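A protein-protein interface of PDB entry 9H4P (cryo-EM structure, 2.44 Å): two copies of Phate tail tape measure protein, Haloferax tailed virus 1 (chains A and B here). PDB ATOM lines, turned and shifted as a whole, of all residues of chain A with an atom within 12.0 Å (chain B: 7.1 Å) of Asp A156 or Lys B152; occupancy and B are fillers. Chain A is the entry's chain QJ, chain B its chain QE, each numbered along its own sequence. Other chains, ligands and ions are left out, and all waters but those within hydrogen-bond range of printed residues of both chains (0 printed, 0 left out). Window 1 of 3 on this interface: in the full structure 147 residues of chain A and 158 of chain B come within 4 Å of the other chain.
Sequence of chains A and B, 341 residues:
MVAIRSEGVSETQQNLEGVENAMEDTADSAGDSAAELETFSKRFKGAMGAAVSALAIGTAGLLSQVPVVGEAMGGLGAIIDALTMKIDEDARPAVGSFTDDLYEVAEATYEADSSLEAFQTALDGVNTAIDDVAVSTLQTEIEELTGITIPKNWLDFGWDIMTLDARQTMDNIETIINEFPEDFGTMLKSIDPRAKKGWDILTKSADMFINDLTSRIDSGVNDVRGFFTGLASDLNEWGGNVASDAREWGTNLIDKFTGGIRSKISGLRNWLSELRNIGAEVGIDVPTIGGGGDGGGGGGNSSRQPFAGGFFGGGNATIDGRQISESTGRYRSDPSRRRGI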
ATOM      1  N   LEU A 145       2.025  11.013 -35.233  1.00  0.00           N
ATOM      2  CA  LEU A 145       1.056  11.932 -34.641  1.00  0.00           C
ATOM      3  C   LEU A 145      -0.357  11.402 -34.863  1.00  0.00           C
ATOM      4  O   LEU A 145      -1.157  11.375 -33.933  1.00  0.00           O
ATOM      5  CB  LEU A 145       1.139  13.313 -35.306  1.00  0.00           C
ATOM      6  CG  LEU A 145       2.029  14.392 -34.687  1.00  0.00           C
ATOM      7  CD1 LEU A 145       2.041  15.616 -35.581  1.00  0.00           C
ATOM      8  CD2 LEU A 145       1.554  14.789 -33.301  1.00  0.00           C
ATOM      9  N   GLY A 147      -1.712   8.669 -37.224  1.00  0.00           N
ATOM     10  CA  GLY A 147      -2.092   7.265 -37.211  1.00  0.00           C
ATOM     11  C   GLY A 147      -2.542   6.819 -35.821  1.00  0.00           C
ATOM     12  O   GLY A 147      -3.459   6.014 -35.700  1.00  0.00           O
ATOM     13  N   ILE A 148      -1.900   7.384 -34.787  1.00  0.00           N
ATOM     14  CA  ILE A 148      -2.236   7.164 -33.389  1.00  0.00           C
ATOM     15  C   ILE A 148      -3.625   7.724 -33.050  1.00  0.00           C
ATOM     16  O   ILE A 148      -4.189   7.352 -32.023  1.00  0.00           O
ATOM     17  CB  ILE A 148      -1.085   7.641 -32.471  1.00  0.00           C
ATOM     18  CG1 ILE A 148       0.138   6.736 -32.640  1.00  0.00           C
ATOM     19  CG2 ILE A 148      -1.510   7.738 -31.016  1.00  0.00           C
ATOM     20  CD1 ILE A 148       1.247   6.942 -31.638  1.00  0.00           C
ATOM     21  N   THR A 149      -4.218   8.555 -33.925  1.00  0.00           N
ATOM     22  CA  THR A 149      -5.581   9.039 -33.716  1.00  0.00           C
ATOM     23  C   THR A 149      -6.628   7.958 -33.996  1.00  0.00           C
ATOM     24  O   THR A 149      -7.753   8.072 -33.514  1.00  0.00           O
ATOM     25  CB  THR A 149      -5.893  10.357 -34.438  1.00  0.00           C
ATOM     26  OG1 THR A 149      -6.048  10.110 -35.836  1.00  0.00           O
ATOM     27  CG2 THR A 149      -4.846  11.421 -34.209  1.00  0.00           C
ATOM     28  N   ILE A 150      -6.265   6.912 -34.752  1.00  0.00           N
ATOM     29  CA  ILE A 150      -7.134   5.759 -34.954  1.00  0.00           C
ATOM     30  C   ILE A 150      -7.347   5.036 -33.617  1.00  0.00           C
ATOM     31  O   ILE A 150      -8.492   4.782 -33.253  1.00  0.00           O
ATOM     32  CB  ILE A 150      -6.645   4.876 -36.124  1.00  0.00           C
ATOM     33  CG1 ILE A 150      -6.797   5.609 -37.460  1.00  0.00           C
ATOM     34  CG2 ILE A 150      -7.346   3.529 -36.145  1.00  0.00           C
ATOM     35  CD1 ILE A 150      -6.034   4.996 -38.605  1.00  0.00           C
ATOM     36  N   PRO A 151      -6.291   4.686 -32.837  1.00  0.00           N
ATOM     37  CA  PRO A 151      -6.447   4.403 -31.409  1.00  0.00           C
ATOM     38  C   PRO A 151      -7.283   5.403 -30.608  1.00  0.00           C
ATOM     39  O   PRO A 151      -8.140   4.972 -29.847  1.00  0.00           O
ATOM     40  CB  PRO A 151      -5.002   4.274 -30.908  1.00  0.00           C
ATOM     41  CG  PRO A 151      -4.262   3.728 -32.097  1.00  0.00           C
ATOM     42  CD  PRO A 151      -4.922   4.388 -33.288  1.00  0.00           C
ATOM     43  N   LYS A 152      -7.081   6.719 -30.794  1.00  0.00           N
ATOM     44  CA  LYS A 152      -7.807   7.732 -30.027  1.00  0.00           C
ATOM     45  C   LYS A 152      -9.307   7.684 -30.334  1.00  0.00           C
ATOM     46  O   LYS A 152     -10.116   8.049 -29.484  1.00  0.00           O
ATOM     47  CB  LYS A 152      -7.267   9.150 -30.259  1.00  0.00           C
ATOM     48  CG  LYS A 152      -5.869   9.446 -29.735  1.00  0.00           C
ATOM     49  CD  LYS A 152      -5.389  10.838 -30.069  1.00  0.00           C
ATOM     50  CE  LYS A 152      -3.942  11.063 -29.699  1.00  0.00           C
ATOM     51  NZ  LYS A 152      -3.492  12.425 -30.062  1.00  0.00           N
ATOM     52  N   ASN A 153      -9.660   7.231 -31.547  1.00  0.00           N
ATOM     53  CA  ASN A 153     -11.031   7.010 -31.980  1.00  0.00           C
ATOM     54  C   ASN A 153     -11.603   5.780 -31.276  1.00  0.00           C
ATOM     55  O   ASN A 153     -12.508   5.906 -30.455  1.00  0.00           O
ATOM     56  CB  ASN A 153     -11.101   6.917 -33.511  1.00  0.00           C
ATOM     57  CG  ASN A 153     -12.492   6.779 -34.099  1.00  0.00           C
ATOM     58  OD1 ASN A 153     -13.444   6.422 -33.413  1.00  0.00           O
ATOM     59  ND2 ASN A 153     -12.619   7.050 -35.385  1.00  0.00           N
ATOM     60  N   TRP A 154     -11.060   4.598 -31.601  1.00  0.00           N
ATOM     61  CA  TRP A 154     -11.685   3.321 -31.279  1.00  0.00           C
ATOM     62  C   TRP A 154     -11.481   2.913 -29.821  1.00  0.00           C
ATOM     63  O   TRP A 154     -12.373   2.299 -29.239  1.00  0.00           O
ATOM     64  CB  TRP A 154     -11.233   2.219 -32.241  1.00  0.00           C
ATOM     65  CG  TRP A 154     -11.471   2.546 -33.682  1.00  0.00           C
ATOM     66  CD1 TRP A 154     -10.522   2.873 -34.600  1.00  0.00           C
ATOM     67  CD2 TRP A 154     -12.730   2.599 -34.381  1.00  0.00           C
ATOM     68  NE1 TRP A 154     -11.098   3.119 -35.815  1.00  0.00           N
ATOM     69  CE2 TRP A 154     -12.453   2.959 -35.714  1.00  0.00           C
ATOM     70  CE3 TRP A 154     -14.065   2.376 -34.021  1.00  0.00           C
ATOM     71  CZ2 TRP A 154     -13.456   3.097 -36.675  1.00  0.00           C
ATOM     72  CZ3 TRP A 154     -15.058   2.512 -34.967  1.00  0.00           C
ATOM     73  CH2 TRP A 154     -14.755   2.870 -36.279  1.00  0.00           C
ATOM     74  N   LEU A 155     -10.313   3.229 -29.241  1.00  0.00           N
ATOM     75  CA  LEU A 155      -9.992   2.779 -27.892  1.00  0.00           C
ATOM     76  C   LEU A 155     -10.778   3.556 -26.836  1.00  0.00           C
ATOM     77  O   LEU A 155     -10.957   3.041 -25.738  1.00  0.00           O
ATOM     78  CB  LEU A 155      -8.486   2.855 -27.606  1.00  0.00           C
ATOM     79  CG  LEU A 155      -7.550   2.000 -28.459  1.00  0.00           C
ATOM     80  CD1 LEU A 155      -6.125   2.113 -27.956  1.00  0.00           C
ATOM     81  CD2 LEU A 155      -7.968   0.541 -28.472  1.00  0.00           C
ATOM     82  N   ASP A 156     -11.256   4.770 -27.156  1.00  0.00           N
ATOM     83  CA  ASP A 156     -11.818   5.667 -26.152  1.00  0.00           C
ATOM     84  C   ASP A 156     -13.249   5.286 -25.772  1.00  0.00           C
ATOM     85  O   ASP A 156     -13.520   5.078 -24.593  1.00  0.00           O
ATOM     86  CB  ASP A 156     -11.566   7.145 -26.466  1.00  0.00           C
ATOM     87  CG  ASP A 156     -10.170   7.633 -26.111  1.00  0.00           C
ATOM     88  OD1 ASP A 156      -9.306   6.796 -25.809  1.00  0.00           O
ATOM     89  OD2 ASP A 156      -9.958   8.854 -26.154  1.00  0.00           O
ATOM     90  N   PHE A 157     -14.156   5.193 -26.750  1.00  0.00           N
ATOM     91  CA  PHE A 157     -15.483   4.673 -26.461  1.00  0.00           C
ATOM     92  C   PHE A 157     -15.385   3.181 -26.162  1.00  0.00           C
ATOM     93  O   PHE A 157     -16.246   2.633 -25.481  1.00  0.00           O
ATOM     94  CB  PHE A 157     -16.484   5.013 -27.568  1.00  0.00           C
ATOM     95  CG  PHE A 157     -16.394   4.204 -28.835  1.00  0.00           C
ATOM     96  CD1 PHE A 157     -15.585   4.613 -29.882  1.00  0.00           C
ATOM     97  CD2 PHE A 157     -17.164   3.063 -29.003  1.00  0.00           C
ATOM     98  CE1 PHE A 157     -15.524   3.884 -31.058  1.00  0.00           C
ATOM     99  CE2 PHE A 157     -17.102   2.335 -30.180  1.00  0.00           C
ATOM    100  CZ  PHE A 157     -16.283   2.747 -31.205  1.00  0.00           C
ATOM    101  N   GLY A 158     -14.329   2.543 -26.682  1.00  0.00           N
ATOM    102  CA  GLY A 158     -13.976   1.169 -26.372  1.00  0.00           C
ATOM    103  C   GLY A 158     -13.733   0.954 -24.880  1.00  0.00           C
ATOM    104  O   GLY A 158     -14.290   0.021 -24.312  1.00  0.00           O
ATOM    105  N   TRP A 159     -12.924   1.824 -24.247  1.00  0.00           N
ATOM    106  CA  TRP A 159     -12.634   1.674 -22.826  1.00  0.00           C
ATOM    107  C   TRP A 159     -13.843   1.935 -21.933  1.00  0.00           C
ATOM    108  O   TRP A 159     -13.858   1.480 -20.793  1.00  0.00           O
ATOM    109  CB  TRP A 159     -11.344   2.351 -22.322  1.00  0.00           C
ATOM    110  CG  TRP A 159     -11.113   3.830 -22.475  1.00  0.00           C
ATOM    111  CD1 TRP A 159     -10.141   4.383 -23.252  1.00  0.00           C
ATOM    112  CD2 TRP A 159     -11.710   4.940 -21.762  1.00  0.00           C
ATOM    113  NE1 TRP A 159     -10.134   5.745 -23.128  1.00  0.00           N
ATOM    114  CE2 TRP A 159     -11.086   6.121 -22.222  1.00  0.00           C
ATOM    115  CE3 TRP A 159     -12.733   5.078 -20.815  1.00  0.00           C
ATOM    116  CZ2 TRP A 159     -11.447   7.394 -21.767  1.00  0.00           C
ATOM    117  CZ3 TRP A 159     -13.089   6.332 -20.362  1.00  0.00           C
ATOM    118  CH2 TRP A 159     -12.455   7.478 -20.835  1.00  0.00           C
ATOM    119  N   ASP A 160     -14.870   2.611 -22.462  1.00  0.00           N
ATOM    120  CA  ASP A 160     -16.142   2.750 -21.765  1.00  0.00           C
ATOM    121  C   ASP A 160     -16.879   1.410 -21.616  1.00  0.00           C
ATOM    122  O   ASP A 160     -17.920   1.368 -20.969  1.00  0.00           O
ATOM    123  CB  ASP A 160     -16.994   3.873 -22.361  1.00  0.00           C
ATOM    124  CG  ASP A 160     -16.570   5.278 -21.975  1.00  0.00           C
ATOM    125  OD1 ASP A 160     -16.159   5.479 -20.824  1.00  0.00           O
ATOM    126  OD2 ASP A 160     -16.677   6.167 -22.830  1.00  0.00           O
ATOM    127  N   ILE A 161     -16.368   0.314 -22.205  1.00  0.00           N
ATOM    128  CA  ILE A 161     -16.772  -1.010 -21.742  1.00  0.00           C
ATOM    129  C   ILE A 161     -15.964  -1.347 -20.489  1.00  0.00           C
ATOM    130  O   ILE A 161     -16.544  -1.635 -19.453  1.00  0.00           O
ATOM    131  CB  ILE A 161     -16.797  -2.140 -22.809  1.00  0.00           C
ATOM    132  CG1 ILE A 161     -15.431  -2.723 -23.178  1.00  0.00           C
ATOM    133  CG2 ILE A 161     -17.596  -1.759 -24.040  1.00  0.00           C
ATOM    134  CD1 ILE A 161     -15.166  -4.075 -22.574  1.00  0.00           C
ATOM    135  N   MET A 162     -14.633  -1.240 -20.572  1.00  0.00           N
ATOM    136  CA  MET A 162     -13.712  -1.664 -19.524  1.00  0.00           C
ATOM    137  C   MET A 162     -13.948  -0.900 -18.219  1.00  0.00           C
ATOM    138  O   MET A 162     -14.218  -1.529 -17.201  1.00  0.00           O
ATOM    139  CB  MET A 162     -12.252  -1.525 -19.973  1.00  0.00           C
ATOM    140  CG  MET A 162     -11.858  -2.442 -21.120  1.00  0.00           C
ATOM    141  SD  MET A 162     -12.003  -4.208 -20.781  1.00  0.00           S
ATOM    142  CE  MET A 162     -10.799  -4.422 -19.476  1.00  0.00           C
ATOM    143  N   THR A 163     -13.858   0.440 -18.256  1.00  0.00           N
ATOM    144  CA  THR A 163     -14.053   1.309 -17.102  1.00  0.00           C
ATOM    145  C   THR A 163     -15.405   1.048 -16.450  1.00  0.00           C
ATOM    146  O   THR A 163     -15.485   0.834 -15.244  1.00  0.00           O
ATOM    147  CB  THR A 163     -14.018   2.792 -17.488  1.00  0.00           C
ATOM    148  OG1 THR A 163     -14.774   2.963 -18.683  1.00  0.00           O
ATOM    149  CG2 THR A 163     -12.628   3.332 -17.717  1.00  0.00           C
ATOM    150  N   LEU A 164     -16.457   1.048 -17.269  1.00  0.00           N
ATOM    151  CA  LEU A 164     -17.808   1.191 -16.756  1.00  0.00           C
ATOM    152  C   LEU A 164     -18.404  -0.163 -16.367  1.00  0.00           C
ATOM    153  O   LEU A 164     -19.094  -0.240 -15.354  1.00  0.00           O
ATOM    154  CB  LEU A 164     -18.669   1.965 -17.760  1.00  0.00           C
ATOM    155  CG  LEU A 164     -18.044   3.219 -18.377  1.00  0.00           C
ATOM    156  CD1 LEU A 164     -19.021   3.930 -19.289  1.00  0.00           C
ATOM    157  CD2 LEU A 164     -17.554   4.184 -17.311  1.00  0.00           C
ATOM    158  N   ASP A 165     -18.122  -1.224 -17.138  1.00  0.00           N
ATOM    159  CA  ASP A 165     -18.721  -2.536 -16.913  1.00  0.00           C
ATOM    160  C   ASP A 165     -18.225  -3.182 -15.621  1.00  0.00           C
ATOM    161  O   ASP A 165     -18.979  -3.904 -14.974  1.00  0.00           O
ATOM    162  CB  ASP A 165     -18.559  -3.477 -18.108  1.00  0.00           C
ATOM    163  CG  ASP A 165     -19.387  -3.088 -19.317  1.00  0.00           C
ATOM    164  OD1 ASP A 165     -20.436  -2.452 -19.137  1.00  0.00           O
ATOM    165  OD2 ASP A 165     -18.981  -3.443 -20.433  1.00  0.00           O
ATOM    166  N   ALA A 166     -16.964  -2.928 -15.257  1.00  0.00           N
ATOM    167  CA  ALA A 166     -16.395  -3.402 -14.006  1.00  0.00           C
ATOM    168  C   ALA A 166     -17.206  -2.883 -12.820  1.00  0.00           C
ATOM    169  O   ALA A 166     -17.250  -3.535 -11.782  1.00  0.00           O
ATOM    170  CB  ALA A 166     -14.952  -2.986 -13.916  1.00  0.00           C
ATOM    171  N   THR B 146       1.694   8.005 -27.002  1.00  0.00           N
ATOM    172  CA  THR B 146       1.525   6.573 -26.782  1.00  0.00           C
ATOM    173  C   THR B 146       1.103   6.331 -25.333  1.00  0.00           C
ATOM    174  O   THR B 146       0.196   5.542 -25.080  1.00  0.00           O
ATOM    175  CB  THR B 146       2.746   5.734 -27.185  1.00  0.00           C
ATOM    176  OG1 THR B 146       3.746   5.853 -26.176  1.00  0.00           O
ATOM    177  CG2 THR B 146       3.326   6.093 -28.536  1.00  0.00           C
ATOM    178  N   GLY B 147       1.749   7.047 -24.401  1.00  0.00           N
ATOM    179  CA  GLY B 147       1.445   7.015 -22.978  1.00  0.00           C
ATOM    180  C   GLY B 147       0.112   7.665 -22.608  1.00  0.00           C
ATOM    181  O   GLY B 147      -0.324   7.541 -21.467  1.00  0.00           O
ATOM    182  N   ILE B 148      -0.522   8.367 -23.557  1.00  0.00           N
ATOM    183  CA  ILE B 148      -1.925   8.734 -23.420  1.00  0.00           C
ATOM    184  C   ILE B 148      -2.798   7.549 -23.850  1.00  0.00           C
ATOM    185  O   ILE B 148      -3.558   7.047 -23.032  1.00  0.00           O
ATOM    186  CB  ILE B 148      -2.260  10.070 -24.125  1.00  0.00           C
ATOM    187  CG1 ILE B 148      -1.656  11.261 -23.379  1.00  0.00           C
ATOM    188  CG2 ILE B 148      -3.760  10.243 -24.320  1.00  0.00           C
ATOM    189  CD1 ILE B 148      -1.741  12.570 -24.127  1.00  0.00           C
ATOM    190  N   THR B 149      -2.649   7.073 -25.097  1.00  0.00           N
ATOM    191  CA  THR B 149      -3.604   6.162 -25.723  1.00  0.00           C
ATOM    192  C   THR B 149      -3.697   4.794 -25.046  1.00  0.00           C
ATOM    193  O   THR B 149      -4.793   4.249 -24.958  1.00  0.00           O
ATOM    194  CB  THR B 149      -3.378   6.005 -27.230  1.00  0.00           C
ATOM    195  OG1 THR B 149      -2.108   5.397 -27.464  1.00  0.00           O
ATOM    196  CG2 THR B 149      -3.478   7.312 -27.982  1.00  0.00           C
ATOM    197  N   ILE B 150      -2.572   4.228 -24.584  1.00  0.00           N
ATOM    198  CA  ILE B 150      -2.571   2.889 -24.006  1.00  0.00           C
ATOM    199  C   ILE B 150      -3.001   2.927 -22.534  1.00  0.00           C
ATOM    200  O   ILE B 150      -3.936   2.216 -22.175  1.00  0.00           O
ATOM    201  CB  ILE B 150      -1.259   2.134 -24.310  1.00  0.00           C
ATOM    202  CG1 ILE B 150      -1.174   1.791 -25.799  1.00  0.00           C
ATOM    203  CG2 ILE B 150      -1.117   0.892 -23.448  1.00  0.00           C
ATOM    204  CD1 ILE B 150       0.198   1.387 -26.274  1.00  0.00           C
ATOM    205  N   PRO B 151      -2.361   3.722 -21.634  1.00  0.00           N
ATOM    206  CA  PRO B 151      -2.915   4.007 -20.308  1.00  0.00           C
ATOM    207  C   PRO B 151      -4.380   4.435 -20.237  1.00  0.00           C
ATOM    208  O   PRO B 151      -5.052   4.087 -19.274  1.00  0.00           O
ATOM    209  CB  PRO B 151      -1.947   5.049 -19.744  1.00  0.00           C
ATOM    210  CG  PRO B 151      -0.638   4.622 -20.331  1.00  0.00           C
ATOM    211  CD  PRO B 151      -1.002   4.273 -21.757  1.00  0.00           C
ATOM    212  N   LYS B 152      -4.880   5.156 -21.248  1.00  0.00           N
ATOM    213  CA  LYS B 152      -6.306   5.445 -21.351  1.00  0.00           C
ATOM    214  C   LYS B 152      -7.131   4.157 -21.345  1.00  0.00           C
ATOM    215  O   LYS B 152      -8.113   4.063 -20.615  1.00  0.00           O
ATOM    216  CB  LYS B 152      -6.622   6.254 -22.611  1.00  0.00           C
ATOM    217  CG  LYS B 152      -6.693   7.763 -22.438  1.00  0.00           C
ATOM    218  CD  LYS B 152      -7.048   8.450 -23.734  1.00  0.00           C
ATOM    219  CE  LYS B 152      -7.478   9.887 -23.554  1.00  0.00           C
ATOM    220  NZ  LYS B 152      -8.026  10.453 -24.808  1.00  0.00           N
ATOM    221  N   ASN B 153      -6.725   3.168 -22.147  1.00  0.00           N
ATOM    222  CA  ASN B 153      -7.490   1.945 -22.356  1.00  0.00           C
ATOM    223  C   ASN B 153      -7.458   1.026 -21.126  1.00  0.00           C
ATOM    224  O   ASN B 153      -8.389   0.244 -20.942  1.00  0.00           O
ATOM    225  CB  ASN B 153      -7.076   1.270 -23.668  1.00  0.00           C
ATOM    226  CG  ASN B 153      -8.035   0.218 -24.183  1.00  0.00           C
ATOM    227  OD1 ASN B 153      -7.745  -0.972 -24.115  1.00  0.00           O
ATOM    228  ND2 ASN B 153      -9.164   0.635 -24.724  1.00  0.00           N
ATOM    229  N   TRP B 154      -6.414   1.128 -20.274  1.00  0.00           N
ATOM    230  CA  TRP B 154      -6.175   0.174 -19.189  1.00  0.00           C
ATOM    231  C   TRP B 154      -6.014   0.797 -17.796  1.00  0.00           C
ATOM    232  O   TRP B 154      -6.486   0.206 -16.829  1.00  0.00           O
ATOM    233  CB  TRP B 154      -5.043  -0.811 -19.525  1.00  0.00           C
ATOM    234  CG  TRP B 154      -5.437  -1.770 -20.605  1.00  0.00           C
ATOM    235  CD1 TRP B 154      -5.228  -1.614 -21.940  1.00  0.00           C
ATOM    236  CD2 TRP B 154      -6.169  -3.003 -20.462  1.00  0.00           C
ATOM    237  NE1 TRP B 154      -5.770  -2.660 -22.635  1.00  0.00           N
ATOM    238  CE2 TRP B 154      -6.364  -3.526 -21.756  1.00  0.00           C
ATOM    239  CE3 TRP B 154      -6.686  -3.720 -19.378  1.00  0.00           C
ATOM    240  CZ2 TRP B 154      -7.039  -4.728 -21.982  1.00  0.00           C
ATOM    241  CZ3 TRP B 154      -7.350  -4.907 -19.601  1.00  0.00           C
ATOM    242  CH2 TRP B 154      -7.530  -5.405 -20.890  1.00  0.00           C
ATOM    243  N   LEU B 155      -5.341   1.952 -17.673  1.00  0.00           N
ATOM    244  CA  LEU B 155      -5.212   2.621 -16.381  1.00  0.00           C
ATOM    245  C   LEU B 155      -6.447   3.459 -16.037  1.00  0.00           C
ATOM    246  O   LEU B 155      -6.793   3.530 -14.862  1.00  0.00           O
ATOM    247  CB  LEU B 155      -3.910   3.425 -16.275  1.00  0.00           C
ATOM    248  CG  LEU B 155      -2.596   2.651 -16.400  1.00  0.00           C
ATOM    249  CD1 LEU B 155      -1.416   3.529 -16.029  1.00  0.00           C
ATOM    250  CD2 LEU B 155      -2.592   1.397 -15.544  1.00  0.00           C
ATOM    251  N   ASP B 156      -7.118   4.084 -17.021  1.00  0.00           N
ATOM    252  CA  ASP B 156      -8.400   4.722 -16.730  1.00  0.00           C
ATOM    253  C   ASP B 156      -9.385   3.661 -16.243  1.00  0.00           C
ATOM    254  O   ASP B 156     -10.130   3.902 -15.298  1.00  0.00           O
ATOM    255  CB  ASP B 156      -8.994   5.510 -17.902  1.00  0.00           C
ATOM    256  CG  ASP B 156      -8.172   6.671 -18.438  1.00  0.00           C
ATOM    257  OD1 ASP B 156      -7.001   6.793 -18.060  1.00  0.00           O
ATOM    258  OD2 ASP B 156      -8.722   7.445 -19.236  1.00  0.00           O
ATOM    259  N   PHE B 157      -9.367   2.491 -16.894  1.00  0.00           N
ATOM    260  CA  PHE B 157     -10.073   1.297 -16.455  1.00  0.00           C
ATOM    261  C   PHE B 157      -9.698   0.972 -15.012  1.00  0.00           C
ATOM    262  O   PHE B 157     -10.571   0.705 -14.196  1.00  0.00           O
ATOM    263  CB  PHE B 157      -9.806   0.153 -17.435  1.00  0.00           C
ATOM    264  CG  PHE B 157      -9.988  -1.250 -16.916  1.00  0.00           C
ATOM    265  CD1 PHE B 157     -11.194  -1.668 -16.378  1.00  0.00           C
ATOM    266  CD2 PHE B 157      -8.956  -2.170 -17.004  1.00  0.00           C
ATOM    267  CE1 PHE B 157     -11.357  -2.966 -15.925  1.00  0.00           C
ATOM    268  CE2 PHE B 157      -9.117  -3.466 -16.543  1.00  0.00           C
ATOM    269  CZ  PHE B 157     -10.318  -3.862 -16.003  1.00  0.00           C
ATOM    270  N   GLY B 158      -8.397   1.022 -14.709  1.00  0.00           N
ATOM    271  CA  GLY B 158      -7.865   0.786 -13.376  1.00  0.00           C
ATOM    272  C   GLY B 158      -8.333   1.805 -12.337  1.00  0.00           C
ATOM    273  O   GLY B 158      -8.378   1.481 -11.154  1.00  0.00           O
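The side-chain amide nitrogen (ND2) of Asn B153 sits at hydrogen-bond distance from the backbone carbonyl oxygen (O) of Leu A155, 3.2 Å away.
The side-chain carboxylate of Asp A156 lies within salt-bridge range of the side-chain amino group of Lys B152, 2.8 Å away.
OG1 of Thr A163 sits at hydrogen-bond distance from O of Trp A159, 2.7 Å away.
The backbone carbonyl oxygen (O) of Pro B151 lies within hydrogen-bond range of the backbone NH (N) of Asp B156, 3.1 Å away.
The side-chain carboxylate (OD1) of Asp A156 sits at hydrogen-bond distance from the indole nitrogen (NE1) of Trp A159, 3.0 Å away.
OD1 of Asn B153 is in hydrogen-bond range of NE1 of Trp B154 (3.0 Å).
The backbone carbonyl oxygen (O) of Thr B146 is in hydrogen-bond range of the side-chain hydroxyl (OG1) of Thr B149 (3.3 Å).
Among the printed residues, pairs that only touch across the chains: Ile A148 with Thr B146 (3.8 Å), Ile A148 with Thr B149 (3.6 Å), Lys A152 with Thr B149 (3.7 Å), Leu A155 with Thr B149 (3.9 Å), Trp A159 with Lys B152 (3.3 Å), Trp A159 with Asn B153 (3.7 Å), Trp A159 with Asp B156 (3.7 Å), Met A162 with Trp B154 (3.5 Å), Met A162 with Phe B157 (3.1 Å), Thr A163 with Asp B156 (3.5 Å) and Thr A163 with Phe B157 (3.5 Å).
Of chain B, only Lys B152 comes within 4 Å of Asp A156.
Of chain A, only Asp A156 and Trp A159 come within 4 Å of Lys B152.
No residue of chain A comes within 4 Å of Ile B148.
No residue of chain A comes within 4 Å of Pro B151.
Asn B153 touches just these residues of chain A: Leu A155 (3.2 Å) and Trp A159 (3.7 Å).
Of the printed residues of chain B, Lys A152 touches Thr B149 (3.7 Å).
Printed residues of chain A within 4 Å of Phe B157: Met A162 (3.1 Å) and Thr A163 (3.5 Å).
Printed residues of chain A within 4 Å of Trp B154: Met A162.
Of the printed residues of chain A, Thr B146 touches Ile A148 (3.8 Å).
Asp A165 touches none of the printed residues of chain B.
Of the 21 printed residues of chain A, 7 touch a printed residue of chain B.
Hydrophobic or aromatic side chains of chain A within 4 Å of the printed part of chain B: Ile A148, Leu A155, Trp A159 and Met A162.
Printed residues of chain B that touch a printed residue of chain A: Thr B146, Thr B149, Lys B152, Asn B153, Trp B154, Asp B156 and Phe B157.
Hydrophobic or aromatic side chains of chain B within 4 Å of the printed part of chain A: Trp B154 and Phe B157.
Among the printed residues, Asp or Glu carboxylates within 4 Å of a Lys or Arg side-chain nitrogen of the other chain: Asp A156 with Lys B152 (2.8 Å).
Ile A148 touches Thr B149, but with the chains exchanged Thr A149 does not touch Ile B148 (9.6 Å).
Lys A152 touches Thr B149, but with the chains exchanged Thr A149 does not touch Lys B152 (9.0 Å).
Leu A155 touches Asn B153, but with the chains exchanged Asn A153 does not touch Leu B155 (15.2 Å).
Asp A156 touches Lys B152, but with the chains exchanged Lys A152 does not touch Asp B156 (10.4 Å).
12 positions are printed for both chains.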
